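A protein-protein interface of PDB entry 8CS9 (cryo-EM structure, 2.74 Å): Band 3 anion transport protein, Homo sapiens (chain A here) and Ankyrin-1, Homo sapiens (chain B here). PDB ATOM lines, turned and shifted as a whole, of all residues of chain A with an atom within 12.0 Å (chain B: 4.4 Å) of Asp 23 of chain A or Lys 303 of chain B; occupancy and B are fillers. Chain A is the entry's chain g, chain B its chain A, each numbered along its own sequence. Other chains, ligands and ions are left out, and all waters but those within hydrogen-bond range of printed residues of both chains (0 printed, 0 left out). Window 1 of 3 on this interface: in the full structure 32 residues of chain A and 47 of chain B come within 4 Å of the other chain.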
ATOM      1  N   GLU A  17      26.066 -22.987 -20.273  1.00  0.00           N
ATOM      2  CA  GLU A  17      27.020 -21.882 -20.386  1.00  0.00           C
ATOM      3  C   GLU A  17      26.917 -20.932 -19.187  1.00  0.00           C
ATOM      4  O   GLU A  17      26.515 -19.773 -19.298  1.00  0.00           O
ATOM      5  CB  GLU A  17      26.822 -21.127 -21.704  1.00  0.00           C
ATOM      6  CG  GLU A  17      27.066 -21.946 -22.950  1.00  0.00           C
ATOM      7  CD  GLU A  17      26.836 -21.149 -24.216  1.00  0.00           C
ATOM      8  OE1 GLU A  17      27.830 -20.707 -24.829  1.00  0.00           O
ATOM      9  OE2 GLU A  17      25.662 -20.957 -24.597  1.00  0.00           O
ATOM     10  N   GLN A  18      27.290 -21.469 -18.023  1.00  0.00           N
ATOM     11  CA  GLN A  18      27.222 -20.699 -16.785  1.00  0.00           C
ATOM     12  C   GLN A  18      28.150 -19.491 -16.787  1.00  0.00           C
ATOM     13  O   GLN A  18      27.948 -18.570 -15.987  1.00  0.00           O
ATOM     14  CB  GLN A  18      27.552 -21.597 -15.594  1.00  0.00           C
ATOM     15  CG  GLN A  18      26.338 -22.224 -14.942  1.00  0.00           C
ATOM     16  CD  GLN A  18      26.680 -23.498 -14.205  1.00  0.00           C
ATOM     17  OE1 GLN A  18      26.381 -24.594 -14.673  1.00  0.00           O
ATOM     18  NE2 GLN A  18      27.311 -23.362 -13.046  1.00  0.00           N
ATOM     19  N   GLU A  19      29.161 -19.469 -17.660  1.00  0.00           N
ATOM     20  CA  GLU A  19      30.096 -18.352 -17.694  1.00  0.00           C
ATOM     21  C   GLU A  19      29.499 -17.103 -18.331  1.00  0.00           C
ATOM     22  O   GLU A  19      30.020 -16.006 -18.112  1.00  0.00           O
ATOM     23  CB  GLU A  19      31.369 -18.755 -18.438  1.00  0.00           C
ATOM     24  N   GLU A  20      28.425 -17.238 -19.107  1.00  0.00           N
ATOM     25  CA  GLU A  20      27.789 -16.084 -19.731  1.00  0.00           C
ATOM     26  C   GLU A  20      26.814 -15.369 -18.807  1.00  0.00           C
ATOM     27  O   GLU A  20      26.227 -14.363 -19.217  1.00  0.00           O
ATOM     28  CB  GLU A  20      27.068 -16.501 -21.014  1.00  0.00           C
ATOM     29  CG  GLU A  20      27.636 -17.739 -21.669  1.00  0.00           C
ATOM     30  CD  GLU A  20      28.802 -17.438 -22.588  1.00  0.00           C
ATOM     31  OE1 GLU A  20      29.191 -16.257 -22.690  1.00  0.00           O
ATOM     32  OE2 GLU A  20      29.332 -18.384 -23.210  1.00  0.00           O
ATOM     33  N   TYR A  21      26.620 -15.862 -17.585  1.00  0.00           N
ATOM     34  CA  TYR A  21      25.835 -15.169 -16.574  1.00  0.00           C
ATOM     35  C   TYR A  21      26.726 -14.533 -15.516  1.00  0.00           C
ATOM     36  O   TYR A  21      26.274 -14.275 -14.396  1.00  0.00           O
ATOM     37  CB  TYR A  21      24.827 -16.122 -15.931  1.00  0.00           C
ATOM     38  CG  TYR A  21      23.910 -16.791 -16.931  1.00  0.00           C
ATOM     39  CD1 TYR A  21      24.271 -17.987 -17.538  1.00  0.00           C
ATOM     40  CD2 TYR A  21      22.693 -16.222 -17.280  1.00  0.00           C
ATOM     41  CE1 TYR A  21      23.447 -18.597 -18.453  1.00  0.00           C
ATOM     42  CE2 TYR A  21      21.859 -16.829 -18.197  1.00  0.00           C
ATOM     43  CZ  TYR A  21      22.243 -18.016 -18.780  1.00  0.00           C
ATOM     44  OH  TYR A  21      21.425 -18.631 -19.697  1.00  0.00           O
ATOM     45  N   GLU A  22      27.986 -14.280 -15.855  1.00  0.00           N
ATOM     46  CA  GLU A  22      28.960 -13.713 -14.938  1.00  0.00           C
ATOM     47  C   GLU A  22      29.591 -12.480 -15.560  1.00  0.00           C
ATOM     48  O   GLU A  22      29.676 -12.358 -16.785  1.00  0.00           O
ATOM     49  CB  GLU A  22      30.062 -14.722 -14.596  1.00  0.00           C
ATOM     50  CG  GLU A  22      29.603 -15.877 -13.736  1.00  0.00           C
ATOM     51  CD  GLU A  22      30.681 -16.924 -13.553  1.00  0.00           C
ATOM     52  OE1 GLU A  22      31.294 -17.332 -14.562  1.00  0.00           O
ATOM     53  OE2 GLU A  22      30.917 -17.337 -12.399  1.00  0.00           O
ATOM     54  N   ASP A  23      30.027 -11.562 -14.705  1.00  0.00           N
ATOM     55  CA  ASP A  23      30.857 -10.453 -15.152  1.00  0.00           C
ATOM     56  C   ASP A  23      32.276 -10.976 -15.340  1.00  0.00           C
ATOM     57  O   ASP A  23      32.962 -11.266 -14.353  1.00  0.00           O
ATOM     58  CB  ASP A  23      30.825  -9.303 -14.144  1.00  0.00           C
ATOM     59  CG  ASP A  23      30.533  -7.969 -14.796  1.00  0.00           C
ATOM     60  OD1 ASP A  23      30.572  -6.942 -14.090  1.00  0.00           O
ATOM     61  OD2 ASP A  23      30.268  -7.949 -16.015  1.00  0.00           O
ATOM     62  N   PRO A  24      32.742 -11.127 -16.588  1.00  0.00           N
ATOM     63  CA  PRO A  24      34.035 -11.788 -16.820  1.00  0.00           C
ATOM     64  C   PRO A  24      35.204 -11.020 -16.230  1.00  0.00           C
ATOM     65  O   PRO A  24      35.943 -11.550 -15.393  1.00  0.00           O
ATOM     66  CB  PRO A  24      34.127 -11.857 -18.352  1.00  0.00           C
ATOM     67  CG  PRO A  24      32.751 -11.514 -18.860  1.00  0.00           C
ATOM     68  CD  PRO A  24      32.157 -10.614 -17.835  1.00  0.00           C
ATOM     69  N   ASP A  25      35.357  -9.764 -16.641  1.00  0.00           N
ATOM     70  CA  ASP A  25      36.437  -8.904 -16.174  1.00  0.00           C
ATOM     71  C   ASP A  25      36.188  -7.500 -16.703  1.00  0.00           C
ATOM     72  O   ASP A  25      35.275  -7.263 -17.499  1.00  0.00           O
ATOM     73  CB  ASP A  25      37.811  -9.409 -16.627  1.00  0.00           C
ATOM     74  N   ILE A  26      37.018  -6.569 -16.245  1.00  0.00           N
ATOM     75  CA  ILE A  26      37.050  -5.209 -16.773  1.00  0.00           C
ATOM     76  C   ILE A  26      38.497  -4.918 -17.150  1.00  0.00           C
ATOM     77  O   ILE A  26      39.201  -4.221 -16.405  1.00  0.00           O
ATOM     78  CB  ILE A  26      36.510  -4.192 -15.755  1.00  0.00           C
ATOM     79  N   PRO A  27      38.980  -5.442 -18.276  1.00  0.00           N
ATOM     80  CA  PRO A  27      40.409  -5.332 -18.590  1.00  0.00           C
ATOM     81  C   PRO A  27      40.843  -3.893 -18.816  1.00  0.00           C
ATOM     82  O   PRO A  27      40.102  -3.068 -19.356  1.00  0.00           O
ATOM     83  CB  PRO A  27      40.556  -6.162 -19.870  1.00  0.00           C
ATOM     84  CG  PRO A  27      39.199  -6.147 -20.487  1.00  0.00           C
ATOM     85  CD  PRO A  27      38.223  -6.111 -19.347  1.00  0.00           C
ATOM     86  N   ASP B 271      27.025 -12.621  -9.753  1.00  0.00           N
ATOM     87  CA  ASP B 271      27.747 -11.437 -10.193  1.00  0.00           C
ATOM     88  C   ASP B 271      26.829 -10.238 -10.396  1.00  0.00           C
ATOM     89  O   ASP B 271      27.205  -9.298 -11.108  1.00  0.00           O
ATOM     90  CB  ASP B 271      28.521 -11.738 -11.476  1.00  0.00           C
ATOM     91  CG  ASP B 271      29.874 -12.362 -11.206  1.00  0.00           C
ATOM     92  OD1 ASP B 271      30.217 -12.553 -10.020  1.00  0.00           O
ATOM     93  OD2 ASP B 271      30.602 -12.658 -12.175  1.00  0.00           O
ATOM     94  N   GLU B 272      25.632 -10.268  -9.803  1.00  0.00           N
ATOM     95  CA  GLU B 272      24.705  -9.133  -9.778  1.00  0.00           C
ATOM     96  C   GLU B 272      24.213  -8.764 -11.176  1.00  0.00           C
ATOM     97  O   GLU B 272      24.090  -7.588 -11.520  1.00  0.00           O
ATOM     98  CB  GLU B 272      25.337  -7.923  -9.085  1.00  0.00           C
ATOM     99  CG  GLU B 272      24.831  -7.679  -7.678  1.00  0.00           C
ATOM    100  CD  GLU B 272      25.733  -6.749  -6.895  1.00  0.00           C
ATOM    101  OE1 GLU B 272      26.965  -6.954  -6.923  1.00  0.00           O
ATOM    102  OE2 GLU B 272      25.214  -5.813  -6.252  1.00  0.00           O
ATOM    103  N   LEU B 273      23.911  -9.775 -11.984  1.00  0.00           N
ATOM    104  CA  LEU B 273      23.354  -9.560 -13.313  1.00  0.00           C
ATOM    105  C   LEU B 273      21.843  -9.739 -13.283  1.00  0.00           C
ATOM    106  O   LEU B 273      21.341 -10.766 -12.818  1.00  0.00           O
ATOM    107  CB  LEU B 273      23.973 -10.519 -14.330  1.00  0.00           C
ATOM    108  CG  LEU B 273      25.199 -10.028 -15.095  1.00  0.00           C
ATOM    109  CD1 LEU B 273      26.460 -10.221 -14.273  1.00  0.00           C
ATOM    110  CD2 LEU B 273      25.313 -10.733 -16.437  1.00  0.00           C
ATOM    111  N   ARG B 281      23.451  -7.848 -23.056  1.00  0.00           N
ATOM    112  CA  ARG B 281      24.771  -8.372 -23.382  1.00  0.00           C
ATOM    113  C   ARG B 281      24.743  -9.169 -24.679  1.00  0.00           C
ATOM    114  O   ARG B 281      25.692  -9.122 -25.469  1.00  0.00           O
ATOM    115  CB  ARG B 281      25.283  -9.230 -22.226  1.00  0.00           C
ATOM    116  CG  ARG B 281      26.640  -9.865 -22.457  1.00  0.00           C
ATOM    117  CD  ARG B 281      26.769 -11.144 -21.659  1.00  0.00           C
ATOM    118  NE  ARG B 281      27.180 -10.885 -20.285  1.00  0.00           N
ATOM    119  CZ  ARG B 281      28.171 -11.515 -19.669  1.00  0.00           C
ATOM    120  NH1 ARG B 281      28.875 -12.455 -20.276  1.00  0.00           N
ATOM    121  NH2 ARG B 281      28.461 -11.192 -18.413  1.00  0.00           N
ATOM    122  N   THR B 302      26.262  -4.404 -12.153  1.00  0.00           N
ATOM    123  CA  THR B 302      26.860  -5.675 -11.785  1.00  0.00           C
ATOM    124  C   THR B 302      27.891  -5.444 -10.681  1.00  0.00           C
ATOM    125  O   THR B 302      27.964  -4.366 -10.087  1.00  0.00           O
ATOM    126  CB  THR B 302      27.474  -6.345 -13.010  1.00  0.00           C
ATOM    127  OG1 THR B 302      28.562  -5.551 -13.499  1.00  0.00           O
ATOM    128  CG2 THR B 302      26.435  -6.494 -14.096  1.00  0.00           C
ATOM    129  N   LYS B 303      28.696  -6.466 -10.383  1.00  0.00           N
ATOM    130  CA  LYS B 303      29.713  -6.322  -9.347  1.00  0.00           C
ATOM    131  C   LYS B 303      30.808  -5.348  -9.761  1.00  0.00           C
ATOM    132  O   LYS B 303      31.436  -4.725  -8.899  1.00  0.00           O
ATOM    133  CB  LYS B 303      30.317  -7.683  -8.998  1.00  0.00           C
ATOM    134  CG  LYS B 303      30.801  -8.479 -10.194  1.00  0.00           C
ATOM    135  CD  LYS B 303      31.778  -9.560  -9.767  1.00  0.00           C
ATOM    136  CE  LYS B 303      32.534 -10.122 -10.957  1.00  0.00           C
ATOM    137  NZ  LYS B 303      33.612 -11.058 -10.539  1.00  0.00           N
ATOM    138  N   ASN B 304      31.048  -5.201 -11.063  1.00  0.00           N
ATOM    139  CA  ASN B 304      32.035  -4.264 -11.582  1.00  0.00           C
ATOM    140  C   ASN B 304      31.422  -2.932 -11.994  1.00  0.00           C
ATOM    141  O   ASN B 304      32.101  -2.120 -12.628  1.00  0.00           O
ATOM    142  CB  ASN B 304      32.778  -4.878 -12.768  1.00  0.00           C
ATOM    143  CG  ASN B 304      33.503  -6.154 -12.405  1.00  0.00           C
ATOM    144  OD1 ASN B 304      33.868  -6.365 -11.249  1.00  0.00           O
ATOM    145  ND2 ASN B 304      33.722  -7.011 -13.392  1.00  0.00           N
ATOM    146  N   GLY B 305      30.159  -2.692 -11.655  1.00  0.00           N
ATOM    147  CA  GLY B 305      29.521  -1.435 -11.984  1.00  0.00           C
ATOM    148  C   GLY B 305      29.085  -1.283 -13.422  1.00  0.00           C
ATOM    149  O   GLY B 305      28.963  -0.153 -13.901  1.00  0.00           O
ATOM    150  N   LEU B 306      28.837  -2.382 -14.129  1.00  0.00           N
ATOM    151  CA  LEU B 306      28.412  -2.325 -15.521  1.00  0.00           C
ATOM    152  C   LEU B 306      26.893  -2.262 -15.595  1.00  0.00           C
ATOM    153  O   LEU B 306      26.201  -3.148 -15.082  1.00  0.00           O
ATOM    154  CB  LEU B 306      28.933  -3.532 -16.298  1.00  0.00           C
ATOM    155  CG  LEU B 306      30.259  -3.353 -17.038  1.00  0.00           C
ATOM    156  CD1 LEU B 306      31.424  -3.590 -16.097  1.00  0.00           C
ATOM    157  CD2 LEU B 306      30.332  -4.280 -18.240  1.00  0.00           C
ATOM    158  N   MET B 311      27.010  -3.439 -21.336  1.00  0.00           N
ATOM    159  CA  MET B 311      27.015  -4.766 -21.940  1.00  0.00           C
ATOM    160  C   MET B 311      26.567  -4.714 -23.394  1.00  0.00           C
ATOM    161  O   MET B 311      27.058  -5.483 -24.227  1.00  0.00           O
ATOM    162  CB  MET B 311      26.127  -5.706 -21.129  1.00  0.00           C
ATOM    163  CG  MET B 311      26.493  -5.769 -19.662  1.00  0.00           C
ATOM    164  SD  MET B 311      26.625  -7.450 -19.039  1.00  0.00           S
ATOM    165  CE  MET B 311      27.411  -7.149 -17.467  1.00  0.00           C
ATOM    166  N   LEU B 336      33.173   0.627 -12.178  1.00  0.00           N
ATOM    167  CA  LEU B 336      34.082   0.827 -11.055  1.00  0.00           C
ATOM    168  C   LEU B 336      35.456   1.289 -11.522  1.00  0.00           C
ATOM    169  O   LEU B 336      36.202   1.896 -10.746  1.00  0.00           O
ATOM    170  CB  LEU B 336      34.193  -0.455 -10.234  1.00  0.00           C
ATOM    171  CG  LEU B 336      32.980  -0.779  -9.361  1.00  0.00           C
ATOM    172  CD1 LEU B 336      33.233  -2.027  -8.538  1.00  0.00           C
ATOM    173  CD2 LEU B 336      32.637   0.395  -8.463  1.00  0.00           C
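OD1 of Asp 271 of chain B is in salt-bridge range of NZ of Lys 303 of chain B (3.7 Å).
The guanidinium group of Arg 281 of chain B lies within hydrogen-bond range of the side-chain sulfur of Met 311 of chain B, 3.7 Å away.
The side-chain hydroxyl (OG1) of Thr 302 of chain B lies close to the backbone NH (N) of Asn 304 of chain B (3.5 Å).
The side-chain hydroxyl (OG1) of Thr 302 of chain B is in hydrogen-bond range of the backbone NH (N) of Leu 306 of chain B (3.2 Å).
The backbone carbonyl oxygen (O) of Asn 304 of chain B lies within hydrogen-bond range of the backbone NH (N) of Leu 336 of chain B, 3.0 Å away.
Glu 22 of chain A touches Asp 271 of chain B (CB to OD2, 3.2 Å).
CD1 of Leu 273 of chain B touches N of Asp 23 of chain A, 3.8 Å away.
Lys 303 of chain B touches Asp 23 of chain A (CE to O, 3.6 Å).
Asp 23 of chain A touches Leu 306 of chain B (OD1 to CD1, 3.999 Å).
Asp 23 of chain A touches Met 311 of chain B.
Pro 24 of chain A touches Arg 281 of chain B (CD to NH2, 3.8 Å).
Hydrophobic or aromatic side chains of chain A within 4 Å of the printed part of chain B: Pro 24.
Of the 11 printed residues of chain B, 8 touch a printed residue of chain A.
Printed residues of chain B that touch a printed residue of chain A: Asp 271, Leu 273, Arg 281, Thr 302, Lys 303, Asn 304, Leu 306 and Met 311.
Among the printed residues, 11 pairs touch across the chains.
Among the printed residues, no Asp or Glu carboxylate lies within 4 Å of a Lys or Arg side-chain nitrogen of the other chain.
The side-chain carboxylate (OD2) of Asp 271 of chain B is in hydrogen-bond range of the backbone NH (N) of Asp 23 of chain A.
The guanidinium group of Arg 281 of chain B sits at hydrogen-bond distance from the backbone carbonyl oxygen of Glu 20 of chain A, 3.4 Å away.
OG1 of Thr 302 of chain B sits at hydrogen-bond distance from OD1 of Asp 23 of chain A (2.5 Å).
The side-chain amide nitrogen of Asn 304 of chain B sits at hydrogen-bond distance from the side-chain carboxylate of Asp 23 of chain A (3.2 Å).
O of Glu 22 of chain A lies close to NH2 of Arg 281 of chain B (2.3 Å).
Printed residues of chain B within 4 Å of Asp 23 of chain A: Asp 271 (2.8 Å), Leu 273 (3.8 Å), Thr 302 (2.5 Å), Lys 303 (3.6 Å), Asn 304 (3.2 Å), Leu 306 (3.999 Å) and Met 311 (3.3 Å).
No residue of chain A comes within 4 Å of Gly 305 of chain B.
Printed residues of chain A within 4 Å of Leu 306 of chain B: Asp 23 (3.999 Å).
Of the printed residues of chain A, Leu 273 of chain B touches Asp 23.
Of the printed residues of chain B, Pro 24 of chain A touches Arg 281 (3.8 Å).
Printed residues of chain B within 4 Å of Glu 20 of chain A: Arg 281 (3.4 Å).
Leu 336 of chain B touches none of the printed residues of chain A.
Pro 27 of chain A touches none of the printed residues of chain B.
The nearest residue of chain A that does not touch Lys 303 of chain B is Pro 24 of chain A (5.4 Å).
The nearest printed residue of chain B that does not touch Pro 24 of chain A is Asn 304 of chain B (5.1 Å).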
